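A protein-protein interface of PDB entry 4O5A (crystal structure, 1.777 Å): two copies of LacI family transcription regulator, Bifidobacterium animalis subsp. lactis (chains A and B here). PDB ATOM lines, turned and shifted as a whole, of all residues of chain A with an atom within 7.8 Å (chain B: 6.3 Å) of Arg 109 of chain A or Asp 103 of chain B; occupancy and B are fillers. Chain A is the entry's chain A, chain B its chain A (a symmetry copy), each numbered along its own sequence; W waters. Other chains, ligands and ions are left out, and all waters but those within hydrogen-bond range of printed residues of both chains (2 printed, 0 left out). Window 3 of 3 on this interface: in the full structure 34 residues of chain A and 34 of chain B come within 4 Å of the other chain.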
ATOM      1  N   ILE A  71     -12.832  -6.036   3.514  1.00  0.00           N
ATOM      2  CA  ILE A  71     -12.796  -6.605   2.177  1.00  0.00           C
ATOM      3  C   ILE A  71     -14.236  -6.940   1.849  1.00  0.00           C
ATOM      4  O   ILE A  71     -14.910  -7.579   2.657  1.00  0.00           O
ATOM      5  CB  ILE A  71     -12.023  -7.942   2.156  1.00  0.00           C
ATOM      6  CG1 ILE A  71     -10.609  -7.769   2.711  1.00  0.00           C
ATOM      7  CG2 ILE A  71     -12.036  -8.555   0.756  1.00  0.00           C
ATOM      8  CD1 ILE A  71      -9.735  -6.823   1.909  1.00  0.00           C
ATOM      9  N   GLY A  72     -14.723  -6.532   0.678  1.00  0.00           N
ATOM     10  CA  GLY A  72     -16.103  -6.836   0.322  1.00  0.00           C
ATOM     11  C   GLY A  72     -16.292  -8.139  -0.438  1.00  0.00           C
ATOM     12  O   GLY A  72     -15.503  -8.477  -1.334  1.00  0.00           O
ATOM     13  N   LEU A  73     -17.345  -8.872  -0.080  1.00  0.00           N
ATOM     14  CA  LEU A  73     -17.723 -10.104  -0.762  1.00  0.00           C
ATOM     15  C   LEU A  73     -19.224 -10.157  -0.894  1.00  0.00           C
ATOM     16  O   LEU A  73     -19.943 -10.109   0.107  1.00  0.00           O
ATOM     17  CB  LEU A  73     -17.231 -11.332   0.021  1.00  0.00           C
ATOM     18  CG  LEU A  73     -17.694 -12.694  -0.500  1.00  0.00           C
ATOM     19  CD1 LEU A  73     -17.244 -12.900  -1.939  1.00  0.00           C
ATOM     20  CD2 LEU A  73     -17.146 -13.793   0.384  1.00  0.00           C
ATOM     21  N   VAL A  74     -19.716 -10.247  -2.126  1.00  0.00           N
ATOM     22  CA  VAL A  74     -21.143 -10.469  -2.319  1.00  0.00           C
ATOM     23  C   VAL A  74     -21.389 -11.940  -2.615  1.00  0.00           C
ATOM     24  O   VAL A  74     -20.823 -12.492  -3.558  1.00  0.00           O
ATOM     25  CB  VAL A  74     -21.730  -9.591  -3.436  1.00  0.00           C
ATOM     26  CG1 VAL A  74     -23.228  -9.816  -3.539  1.00  0.00           C
ATOM     27  CG2 VAL A  74     -21.460  -8.123  -3.145  1.00  0.00           C
ATOM     28  N   LEU A  75     -22.208 -12.576  -1.786  1.00  0.00           N
ATOM     29  CA  LEU A  75     -22.573 -13.976  -2.002  1.00  0.00           C
ATOM     30  C   LEU A  75     -23.935 -14.085  -2.673  1.00  0.00           C
ATOM     31  O   LEU A  75     -24.747 -13.158  -2.605  1.00  0.00           O
ATOM     32  CB  LEU A  75     -22.594 -14.736  -0.677  1.00  0.00           C
ATOM     33  CG  LEU A  75     -21.267 -14.860   0.063  1.00  0.00           C
ATOM     34  CD1 LEU A  75     -21.470 -15.545   1.408  1.00  0.00           C
ATOM     35  CD2 LEU A  75     -20.290 -15.633  -0.790  1.00  0.00           C
ATOM     36  N   GLY A  76     -24.199 -15.217  -3.318  1.00  0.00           N
ATOM     37  CA  GLY A  76     -25.497 -15.425  -3.934  1.00  0.00           C
ATOM     38  C   GLY A  76     -26.435 -16.113  -2.964  1.00  0.00           C
ATOM     39  O   GLY A  76     -26.016 -17.015  -2.238  1.00  0.00           O
ATOM     40  N   TYR A  77     -27.697 -15.694  -2.935  1.00  0.00           N
ATOM     41  CA  TYR A  77     -28.669 -16.305  -2.033  1.00  0.00           C
ATOM     42  C   TYR A  77     -28.899 -17.770  -2.404  1.00  0.00           C
ATOM     43  O   TYR A  77     -29.146 -18.091  -3.571  1.00  0.00           O
ATOM     44  CB  TYR A  77     -29.992 -15.539  -2.049  1.00  0.00           C
ATOM     45  CG  TYR A  77     -31.046 -16.129  -1.136  1.00  0.00           C
ATOM     46  CD1 TYR A  77     -30.930 -16.032   0.247  1.00  0.00           C
ATOM     47  CD2 TYR A  77     -32.155 -16.781  -1.653  1.00  0.00           C
ATOM     48  CE1 TYR A  77     -31.894 -16.566   1.087  1.00  0.00           C
ATOM     49  CE2 TYR A  77     -33.121 -17.322  -0.821  1.00  0.00           C
ATOM     50  CZ  TYR A  77     -32.984 -17.210   0.548  1.00  0.00           C
ATOM     51  OH  TYR A  77     -33.946 -17.746   1.375  1.00  0.00           O
ATOM     52  N   LEU A 106     -14.167  -9.209   6.854  1.00  0.00           N
ATOM     53  CA  LEU A 106     -14.856  -9.444   5.594  1.00  0.00           C
ATOM     54  C   LEU A 106     -16.253  -8.834   5.701  1.00  0.00           C
ATOM     55  O   LEU A 106     -16.986  -9.116   6.663  1.00  0.00           O
ATOM     56  CB  LEU A 106     -14.991 -10.947   5.374  1.00  0.00           C
ATOM     57  CG  LEU A 106     -15.410 -11.468   4.003  1.00  0.00           C
ATOM     58  CD1 LEU A 106     -14.281 -11.262   2.997  1.00  0.00           C
ATOM     59  CD2 LEU A 106     -15.791 -12.953   4.092  1.00  0.00           C
ATOM     60  N   LEU A 107     -16.628  -8.011   4.728  1.00  0.00           N
ATOM     61  CA  LEU A 107     -17.963  -7.427   4.718  1.00  0.00           C
ATOM     62  C   LEU A 107     -18.800  -8.216   3.713  1.00  0.00           C
ATOM     63  O   LEU A 107     -18.483  -8.246   2.523  1.00  0.00           O
ATOM     64  CB  LEU A 107     -17.904  -5.949   4.328  1.00  0.00           C
ATOM     65  CG  LEU A 107     -19.211  -5.177   4.536  1.00  0.00           C
ATOM     66  CD1 LEU A 107     -19.494  -4.979   6.020  1.00  0.00           C
ATOM     67  CD2 LEU A 107     -19.180  -3.840   3.813  1.00  0.00           C
ATOM     68  N   VAL A 108     -19.856  -8.862   4.197  1.00  0.00           N
ATOM     69  CA  VAL A 108     -20.623  -9.788   3.371  1.00  0.00           C
ATOM     70  C   VAL A 108     -22.012  -9.258   3.086  1.00  0.00           C
ATOM     71  O   VAL A 108     -22.766  -8.913   4.005  1.00  0.00           O
ATOM     72  CB  VAL A 108     -20.744 -11.157   4.044  1.00  0.00           C
ATOM     73  CG1 VAL A 108     -21.633 -12.094   3.210  1.00  0.00           C
ATOM     74  CG2 VAL A 108     -19.372 -11.765   4.248  1.00  0.00           C
ATOM     75  N   ARG A 109     -22.353  -9.185   1.802  1.00  0.00           N
ATOM     76  CA  ARG A 109     -23.722  -8.912   1.412  1.00  0.00           C
ATOM     77  C   ARG A 109     -24.241 -10.025   0.512  1.00  0.00           C
ATOM     78  O   ARG A 109     -23.483 -10.891   0.092  1.00  0.00           O
ATOM     79  CB  ARG A 109     -23.868  -7.524   0.779  1.00  0.00           C
ATOM     80  CG  ARG A 109     -23.870  -6.426   1.837  1.00  0.00           C
ATOM     81  CD  ARG A 109     -24.347  -5.080   1.329  1.00  0.00           C
ATOM     82  NE  ARG A 109     -25.714  -5.094   0.836  1.00  0.00           N
ATOM     83  CZ  ARG A 109     -26.409  -3.991   0.570  1.00  0.00           C
ATOM     84  NH1 ARG A 109     -25.855  -2.802   0.766  1.00  0.00           N
ATOM     85  NH2 ARG A 109     -27.652  -4.070   0.118  1.00  0.00           N
ATOM     86  N   MET A 110     -25.535 -10.010   0.243  1.00  0.00           N
ATOM     87  CA  MET A 110     -26.187 -11.150  -0.386  1.00  0.00           C
ATOM     88  C   MET A 110     -26.975 -10.643  -1.579  1.00  0.00           C
ATOM     89  O   MET A 110     -27.848  -9.788  -1.430  1.00  0.00           O
ATOM     90  CB  MET A 110     -27.119 -11.826   0.640  1.00  0.00           C
ATOM     91  CG  MET A 110     -27.725 -13.191   0.257  1.00  0.00           C
ATOM     92  SD  MET A 110     -26.493 -14.709   0.402  1.00  0.00           S
ATOM     93  CE  MET A 110     -25.489 -14.162   1.966  1.00  0.00           C
ATOM     94  N   SER A 111     -26.673 -11.152  -2.771  1.00  0.00           N
ATOM     95  CA  SER A 111     -27.483 -10.795  -3.934  1.00  0.00           C
ATOM     96  C   SER A 111     -28.653 -11.772  -4.095  1.00  0.00           C
ATOM     97  O   SER A 111     -28.474 -12.994  -4.100  1.00  0.00           O
ATOM     98  CB  SER A 111     -26.639 -10.710  -5.209  1.00  0.00           C
ATOM     99  OG  SER A 111     -26.280 -11.991  -5.678  1.00  0.00           O
ATOM    100  N   MET A 112     -29.855 -11.223  -4.196  1.00  0.00           N
ATOM    101  CA  MET A 112     -31.073 -12.034  -4.247  1.00  0.00           C
ATOM    102  C   MET A 112     -31.518 -12.224  -5.690  1.00  0.00           C
ATOM    103  O   MET A 112     -32.383 -13.056  -5.983  1.00  0.00           O
ATOM    104  CB  MET A 112     -32.197 -11.369  -3.442  1.00  0.00           C
ATOM    105  CG  MET A 112     -31.780 -10.868  -2.061  1.00  0.00           C
ATOM    106  SD  MET A 112     -31.271 -12.288  -0.813  1.00  0.00           S
ATOM    107  CE  MET A 112     -32.985 -13.214  -0.743  1.00  0.00           C
ATOM    108  N   ASP A 116     -28.376  -7.730  -8.971  1.00  0.00           N
ATOM    109  CA  ASP A 116     -28.262  -7.260  -7.593  1.00  0.00           C
ATOM    110  C   ASP A 116     -26.796  -7.095  -7.188  1.00  0.00           C
ATOM    111  O   ASP A 116     -26.434  -6.126  -6.509  1.00  0.00           O
ATOM    112  CB  ASP A 116     -28.953  -8.263  -6.657  1.00  0.00           C
ATOM    113  CG  ASP A 116     -29.380  -7.647  -5.331  1.00  0.00           C
ATOM    114  OD1 ASP A 116     -29.007  -6.489  -5.048  1.00  0.00           O
ATOM    115  OD2 ASP A 116     -30.089  -8.337  -4.564  1.00  0.00           O
ATOM    116  N   SER A 119     -25.198  -3.873  -8.520  1.00  0.00           N
ATOM    117  CA  SER A 119     -25.700  -2.725  -7.771  1.00  0.00           C
ATOM    118  C   SER A 119     -25.011  -2.554  -6.412  1.00  0.00           C
ATOM    119  O   SER A 119     -24.642  -1.448  -6.032  1.00  0.00           O
ATOM    120  CB  SER A 119     -27.216  -2.820  -7.605  1.00  0.00           C
ATOM    121  OG  SER A 119     -27.708  -1.709  -6.888  1.00  0.00           O
ATOM    122  N   ILE A 120     -24.820  -3.652  -5.688  1.00  0.00           N
ATOM    123  CA  ILE A 120     -24.141  -3.587  -4.399  1.00  0.00           C
ATOM    124  C   ILE A 120     -22.688  -3.144  -4.569  1.00  0.00           C
ATOM    125  O   ILE A 120     -22.190  -2.304  -3.816  1.00  0.00           O
ATOM    126  CB  ILE A 120     -24.206  -4.941  -3.669  1.00  0.00           C
ATOM    127  CG1 ILE A 120     -25.661  -5.273  -3.316  1.00  0.00           C
ATOM    128  CG2 ILE A 120     -23.329  -4.925  -2.421  1.00  0.00           C
ATOM    129  CD1 ILE A 120     -25.888  -6.714  -2.891  1.00  0.00           C
ATOM    130  N   LEU A 121     -22.021  -3.701  -5.577  1.00  0.00           N
ATOM    131  CA  LEU A 121     -20.626  -3.388  -5.852  1.00  0.00           C
ATOM    132  C   LEU A 121     -20.477  -1.918  -6.218  1.00  0.00           C
ATOM    133  O   LEU A 121     -19.535  -1.256  -5.787  1.00  0.00           O
ATOM    134  CB  LEU A 121     -20.109  -4.264  -6.991  1.00  0.00           C
ATOM    135  CG  LEU A 121     -19.972  -5.757  -6.699  1.00  0.00           C
ATOM    136  CD1 LEU A 121     -19.446  -6.499  -7.922  1.00  0.00           C
ATOM    137  CD2 LEU A 121     -19.081  -6.002  -5.488  1.00  0.00           C
ATOM    138  N   ASP A 123     -22.314   0.462  -5.209  1.00  0.00           N
ATOM    139  CA  ASP A 123     -22.513   1.235  -3.990  1.00  0.00           C
ATOM    140  C   ASP A 123     -21.225   1.268  -3.177  1.00  0.00           C
ATOM    141  O   ASP A 123     -20.819   2.320  -2.683  1.00  0.00           O
ATOM    142  CB  ASP A 123     -23.665   0.649  -3.165  1.00  0.00           C
ATOM    143  CG  ASP A 123     -23.791   1.293  -1.797  1.00  0.00           C
ATOM    144  OD1 ASP A 123     -24.269   2.447  -1.721  1.00  0.00           O
ATOM    145  OD2 ASP A 123     -23.418   0.641  -0.797  1.00  0.00           O
ATOM    146  N   TRP A 124     -20.583   0.109  -3.058  1.00  0.00           N
ATOM    147  CA  TRP A 124     -19.343  -0.012  -2.306  1.00  0.00           C
ATOM    148  C   TRP A 124     -18.257   0.851  -2.924  1.00  0.00           C
ATOM    149  O   TRP A 124     -17.498   1.507  -2.217  1.00  0.00           O
ATOM    150  CB  TRP A 124     -18.903  -1.472  -2.259  1.00  0.00           C
ATOM    151  CG  TRP A 124     -19.591  -2.250  -1.186  1.00  0.00           C
ATOM    152  CD1 TRP A 124     -20.403  -1.756  -0.203  1.00  0.00           C
ATOM    153  CD2 TRP A 124     -19.526  -3.667  -0.982  1.00  0.00           C
ATOM    154  NE1 TRP A 124     -20.848  -2.785   0.604  1.00  0.00           N
ATOM    155  CE2 TRP A 124     -20.319  -3.964   0.150  1.00  0.00           C
ATOM    156  CE3 TRP A 124     -18.874  -4.712  -1.640  1.00  0.00           C
ATOM    157  CZ2 TRP A 124     -20.474  -5.267   0.630  1.00  0.00           C
ATOM    158  CZ3 TRP A 124     -19.033  -6.002  -1.164  1.00  0.00           C
ATOM    159  CH2 TRP A 124     -19.828  -6.268  -0.040  1.00  0.00           C
ATOM    160  N   ASN A 129     -16.593   1.985   0.736  1.00  0.00           N
ATOM    161  CA  ASN A 129     -16.956   1.333   1.987  1.00  0.00           C
ATOM    162  C   ASN A 129     -16.110   0.112   2.313  1.00  0.00           C
ATOM    163  O   ASN A 129     -16.177  -0.419   3.426  1.00  0.00           O
ATOM    164  CB  ASN A 129     -18.438   0.958   1.987  1.00  0.00           C
ATOM    165  CG  ASN A 129     -18.970   0.726   3.380  1.00  0.00           C
ATOM    166  OD1 ASN A 129     -18.733   1.530   4.282  1.00  0.00           O
ATOM    167  ND2 ASN A 129     -19.671  -0.387   3.574  1.00  0.00           N
ATOM    168  N   ARG B  69     -24.893   0.242   9.934  1.00  0.00           N
ATOM    169  CA  ARG B  69     -25.559  -0.704   9.039  1.00  0.00           C
ATOM    170  C   ARG B  69     -24.799  -2.015   8.900  1.00  0.00           C
ATOM    171  O   ARG B  69     -24.804  -2.633   7.836  1.00  0.00           O
ATOM    172  CB  ARG B  69     -25.858  -0.079   7.671  1.00  0.00           C
ATOM    173  CG  ARG B  69     -26.543   1.279   7.782  1.00  0.00           C
ATOM    174  CD  ARG B  69     -27.207   1.694   6.480  1.00  0.00           C
ATOM    175  NE  ARG B  69     -28.523   1.073   6.357  1.00  0.00           N
ATOM    176  CZ  ARG B  69     -29.631   1.536   6.938  1.00  0.00           C
ATOM    177  NH1 ARG B  69     -30.780   0.896   6.778  1.00  0.00           N
ATOM    178  NH2 ARG B  69     -29.594   2.636   7.684  1.00  0.00           N
ATOM    179  N   GLY B  96     -28.798 -12.765   5.509  1.00  0.00           N
ATOM    180  CA  GLY B  96     -28.714 -11.853   4.384  1.00  0.00           C
ATOM    181  C   GLY B  96     -30.049 -11.536   3.738  1.00  0.00           C
ATOM    182  O   GLY B  96     -30.253 -10.413   3.280  1.00  0.00           O
ATOM    183  N   ALA B  98     -32.763 -11.032   5.093  1.00  0.00           N
ATOM    184  CA  ALA B  98     -33.431  -9.985   5.861  1.00  0.00           C
ATOM    185  C   ALA B  98     -32.611  -8.697   5.940  1.00  0.00           C
ATOM    186  O   ALA B  98     -33.175  -7.598   5.862  1.00  0.00           O
ATOM    187  CB  ALA B  98     -33.810 -10.477   7.257  1.00  0.00           C
ATOM    188  N   LEU B  99     -31.297  -8.823   6.092  1.00  0.00           N
ATOM    189  CA  LEU B  99     -30.435  -7.640   6.166  1.00  0.00           C
ATOM    190  C   LEU B  99     -30.481  -6.838   4.868  1.00  0.00           C
ATOM    191  O   LEU B  99     -30.420  -5.611   4.902  1.00  0.00           O
ATOM    192  CB  LEU B  99     -28.991  -8.020   6.513  1.00  0.00           C
ATOM    193  CG  LEU B  99     -28.823  -8.717   7.862  1.00  0.00           C
ATOM    194  CD1 LEU B  99     -27.382  -9.181   8.014  1.00  0.00           C
ATOM    195  CD2 LEU B  99     -29.239  -7.782   9.016  1.00  0.00           C
ATOM    196  N   GLU B 100     -30.625  -7.526   3.731  1.00  0.00           N
ATOM    197  CA  GLU B 100     -30.669  -6.831   2.437  1.00  0.00           C
ATOM    198  C   GLU B 100     -31.880  -5.926   2.304  1.00  0.00           C
ATOM    199  O   GLU B 100     -31.820  -4.907   1.611  1.00  0.00           O
ATOM    200  CB  GLU B 100     -30.656  -7.818   1.271  1.00  0.00           C
ATOM    201  CG  GLU B 100     -29.299  -8.451   1.020  1.00  0.00           C
ATOM    202  CD  GLU B 100     -28.266  -7.451   0.543  1.00  0.00           C
ATOM    203  OE1 GLU B 100     -28.631  -6.534  -0.230  1.00  0.00           O
ATOM    204  OE2 GLU B 100     -27.080  -7.583   0.937  1.00  0.00           O
ATOM    205  N   GLU B 101     -32.975  -6.305   2.958  1.00  0.00           N
ATOM    206  CA  GLU B 101     -34.192  -5.488   2.947  1.00  0.00           C
ATOM    207  C   GLU B 101     -33.960  -4.101   3.537  1.00  0.00           C
ATOM    208  O   GLU B 101     -34.700  -3.167   3.221  1.00  0.00           O
ATOM    209  CB  GLU B 101     -35.328  -6.196   3.712  1.00  0.00           C
ATOM    210  CG  GLU B 101     -35.793  -7.488   3.071  1.00  0.00           C
ATOM    211  CD  GLU B 101     -36.936  -8.151   3.824  1.00  0.00           C
ATOM    212  OE1 GLU B 101     -37.933  -7.469   4.139  1.00  0.00           O
ATOM    213  OE2 GLU B 101     -36.845  -9.365   4.090  1.00  0.00           O
ATOM    214  N   ARG B 102     -32.949  -3.967   4.397  1.00  0.00           N
ATOM    215  CA  ARG B 102     -32.656  -2.694   5.060  1.00  0.00           C
ATOM    216  C   ARG B 102     -31.258  -2.199   4.703  1.00  0.00           C
ATOM    217  O   ARG B 102     -30.723  -1.318   5.381  1.00  0.00           O
ATOM    218  CB  ARG B 102     -32.697  -2.860   6.586  1.00  0.00           C
ATOM    219  CG  ARG B 102     -33.943  -3.515   7.155  1.00  0.00           C
ATOM    220  CD  ARG B 102     -35.002  -2.486   7.477  1.00  0.00           C
ATOM    221  NE  ARG B 102     -34.507  -1.420   8.352  1.00  0.00           N
ATOM    222  CZ  ARG B 102     -34.713  -1.349   9.668  1.00  0.00           C
ATOM    223  NH1 ARG B 102     -35.417  -2.281  10.292  1.00  0.00           N
ATOM    224  NH2 ARG B 102     -34.224  -0.327  10.363  1.00  0.00           N
ATOM    225  N   ASP B 103     -30.663  -2.791   3.669  1.00  0.00           N
ATOM    226  CA  ASP B 103     -29.319  -2.404   3.218  1.00  0.00           C
ATOM    227  C   ASP B 103     -28.260  -2.539   4.324  1.00  0.00           C
ATOM    228  O   ASP B 103     -27.360  -1.713   4.477  1.00  0.00           O
ATOM    229  CB  ASP B 103     -29.341  -1.018   2.591  1.00  0.00           C
ATOM    230  CG  ASP B 103     -30.166  -0.988   1.319  1.00  0.00           C
ATOM    231  OD1 ASP B 103     -29.791  -1.695   0.353  1.00  0.00           O
ATOM    232  OD2 ASP B 103     -31.199  -0.291   1.292  1.00  0.00           O
ATOM    233  N   TYR B 104     -28.391  -3.606   5.096  1.00  0.00           N
ATOM    234  CA  TYR B 104     -27.439  -3.922   6.139  1.00  0.00           C
ATOM    235  C   TYR B 104     -26.464  -4.953   5.594  1.00  0.00           C
ATOM    236  O   TYR B 104     -26.788  -5.674   4.647  1.00  0.00           O
ATOM    237  CB  TYR B 104     -28.179  -4.494   7.354  1.00  0.00           C
ATOM    238  CG  TYR B 104     -28.358  -3.485   8.461  1.00  0.00           C
ATOM    239  CD1 TYR B 104     -29.173  -2.384   8.294  1.00  0.00           C
ATOM    240  CD2 TYR B 104     -27.695  -3.631   9.672  1.00  0.00           C
ATOM    241  CE1 TYR B 104     -29.332  -1.448   9.303  1.00  0.00           C
ATOM    242  CE2 TYR B 104     -27.851  -2.703  10.691  1.00  0.00           C
ATOM    243  CZ  TYR B 104     -28.666  -1.619  10.496  1.00  0.00           C
ATOM    244  OH  TYR B 104     -28.830  -0.681  11.488  1.00  0.00           O
ATOM    245  N   SER B 105     -25.282  -5.025   6.204  1.00  0.00           N
ATOM    246  CA  SER B 105     -24.254  -6.004   5.831  1.00  0.00           C
ATOM    247  C   SER B 105     -23.867  -6.815   7.054  1.00  0.00           C
ATOM    248  O   SER B 105     -24.084  -6.389   8.187  1.00  0.00           O
ATOM    249  CB  SER B 105     -22.981  -5.308   5.327  1.00  0.00           C
ATOM    250  OG  SER B 105     -23.218  -4.467   4.224  1.00  0.00           O
ATOM    251  N   LEU B 106     -23.262  -7.974   6.823  1.00  0.00           N
ATOM    252  CA  LEU B 106     -22.713  -8.773   7.908  1.00  0.00           C
ATOM    253  C   LEU B 106     -21.202  -8.543   7.942  1.00  0.00           C
ATOM    254  O   LEU B 106     -20.526  -8.679   6.911  1.00  0.00           O
ATOM    255  CB  LEU B 106     -22.980 -10.247   7.625  1.00  0.00           C
ATOM    256  CG  LEU B 106     -22.770 -11.272   8.735  1.00  0.00           C
ATOM    257  CD1 LEU B 106     -23.851 -11.117   9.803  1.00  0.00           C
ATOM    258  CD2 LEU B 106     -22.782 -12.694   8.155  1.00  0.00           C
HETATM  259  O   HOH W   1     -29.913  -5.043  -2.502  1.00  0.00           O
HETATM  260  O   HOH W   2     -23.443  -2.008   2.095  1.00  0.00           O
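The backbone NH of Met 110 of chain A lies within hydrogen-bond range of the side-chain carboxylate of Glu 100 of chain B (3.0 Å). The side-chain carboxylate (OE1) of Glu 100 of chain B lies within salt-bridge range of the guanidinium group (NH2) of Arg 109 of chain A (2.7 Å). The guanidinium group (NH2) of Arg 109 of chain A lies within salt-bridge range of the side-chain carboxylate (OD1) of Asp 103 of chain B (3.2 Å). The backbone NH of Val 108 of chain A is in hydrogen-bond range of the backbone carbonyl oxygen of Leu 106 of chain B.
The backbone NH (N) of Tyr 77 of chain A lies close to the side-chain sulfur (SD) of Met 110 of chain A, at 3.7 Å. The backbone carbonyl oxygen of Arg 69 of chain B sits at hydrogen-bond distance from the backbone NH of Ser 105 of chain B (2.9 Å). The backbone carbonyl oxygen (O) of Leu 73 of chain A is in hydrogen-bond range of the backbone NH (N) of Arg 109 of chain A (3.1 Å). The backbone carbonyl oxygen (O) of Leu 107 of chain A is in hydrogen-bond range of the backbone NH (N) of Leu 73 of chain A (2.9 Å). N of Leu 75 of chain A sits at hydrogen-bond distance from O of Arg 109 of chain A (2.8 Å). The backbone NH (N) of Leu 107 of chain A sits at hydrogen-bond distance from the backbone carbonyl oxygen (O) of Ile 71 of chain A (2.7 Å).
Leu 106 of chain A touches Leu 106 of chain B (O to O, 3.6 Å). CD1 of Leu 107 of chain A touches CB of Ser 105 of chain B, at 3.6 Å. Leu 106 of chain B touches Leu 107 of chain A. Val 108 of chain A touches Ser 105 of chain B (O to CA, 3.7 Å). Ser 105 of chain B touches Arg 109 of chain A. OE1 of Glu 100 of chain B touches CD1 of Ile 120 of chain A, at 3.8 Å.
Val 74 of chain A touches none of the printed residues of chain B. Printed residues of chain B within 4 Å of Leu 107 of chain A: Ser 105 and Leu 106. Printed residues of chain B within 4 Å of Arg 109 of chain A: Glu 100 (2.7 Å), Asp 103 (3.2 Å) and Ser 105 (3.2 Å). Printed residues of chain B within 4 Å of Met 110 of chain A: Glu 100 (3.0 Å). Printed residues of chain B within 4 Å of Ile 120 of chain A: Glu 100. Leu 121 of chain A touches none of the printed residues of chain B. Of the printed residues of chain A, Glu 100 of chain B touches Arg 109, Met 110 and Ile 120. Of chain A, only Arg 109 comes within 4 Å of Asp 103 of chain B. Printed residues of chain A within 4 Å of Ser 105 of chain B: Leu 107, Val 108 and Arg 109.
Hydrophobic or aromatic side chains of chain A within 4 Å of the printed part of chain B: Leu 107, Val 108 and Ile 120. Of the 11 printed residues of chain B, 4 touch a printed residue of chain A. Among the printed residues, 10 pairs touch across the chains.
Leu 106 of chain B touches its own counterpart, Leu 106 of chain A. 1 position is printed for both chains.
Water W2 lies within hydrogen-bond range of the guanidinium group of Arg 109 of chain A (2.9 Å), the indole nitrogen of Trp 124 of chain A (3.1 Å) and the side-chain hydroxyl of Ser 105 of chain B (3.3 Å). Water W1 bridges OE1 of Glu 100 of chain B (3.0 Å) and OD1 of Asp 116 of chain A (3.1 Å).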
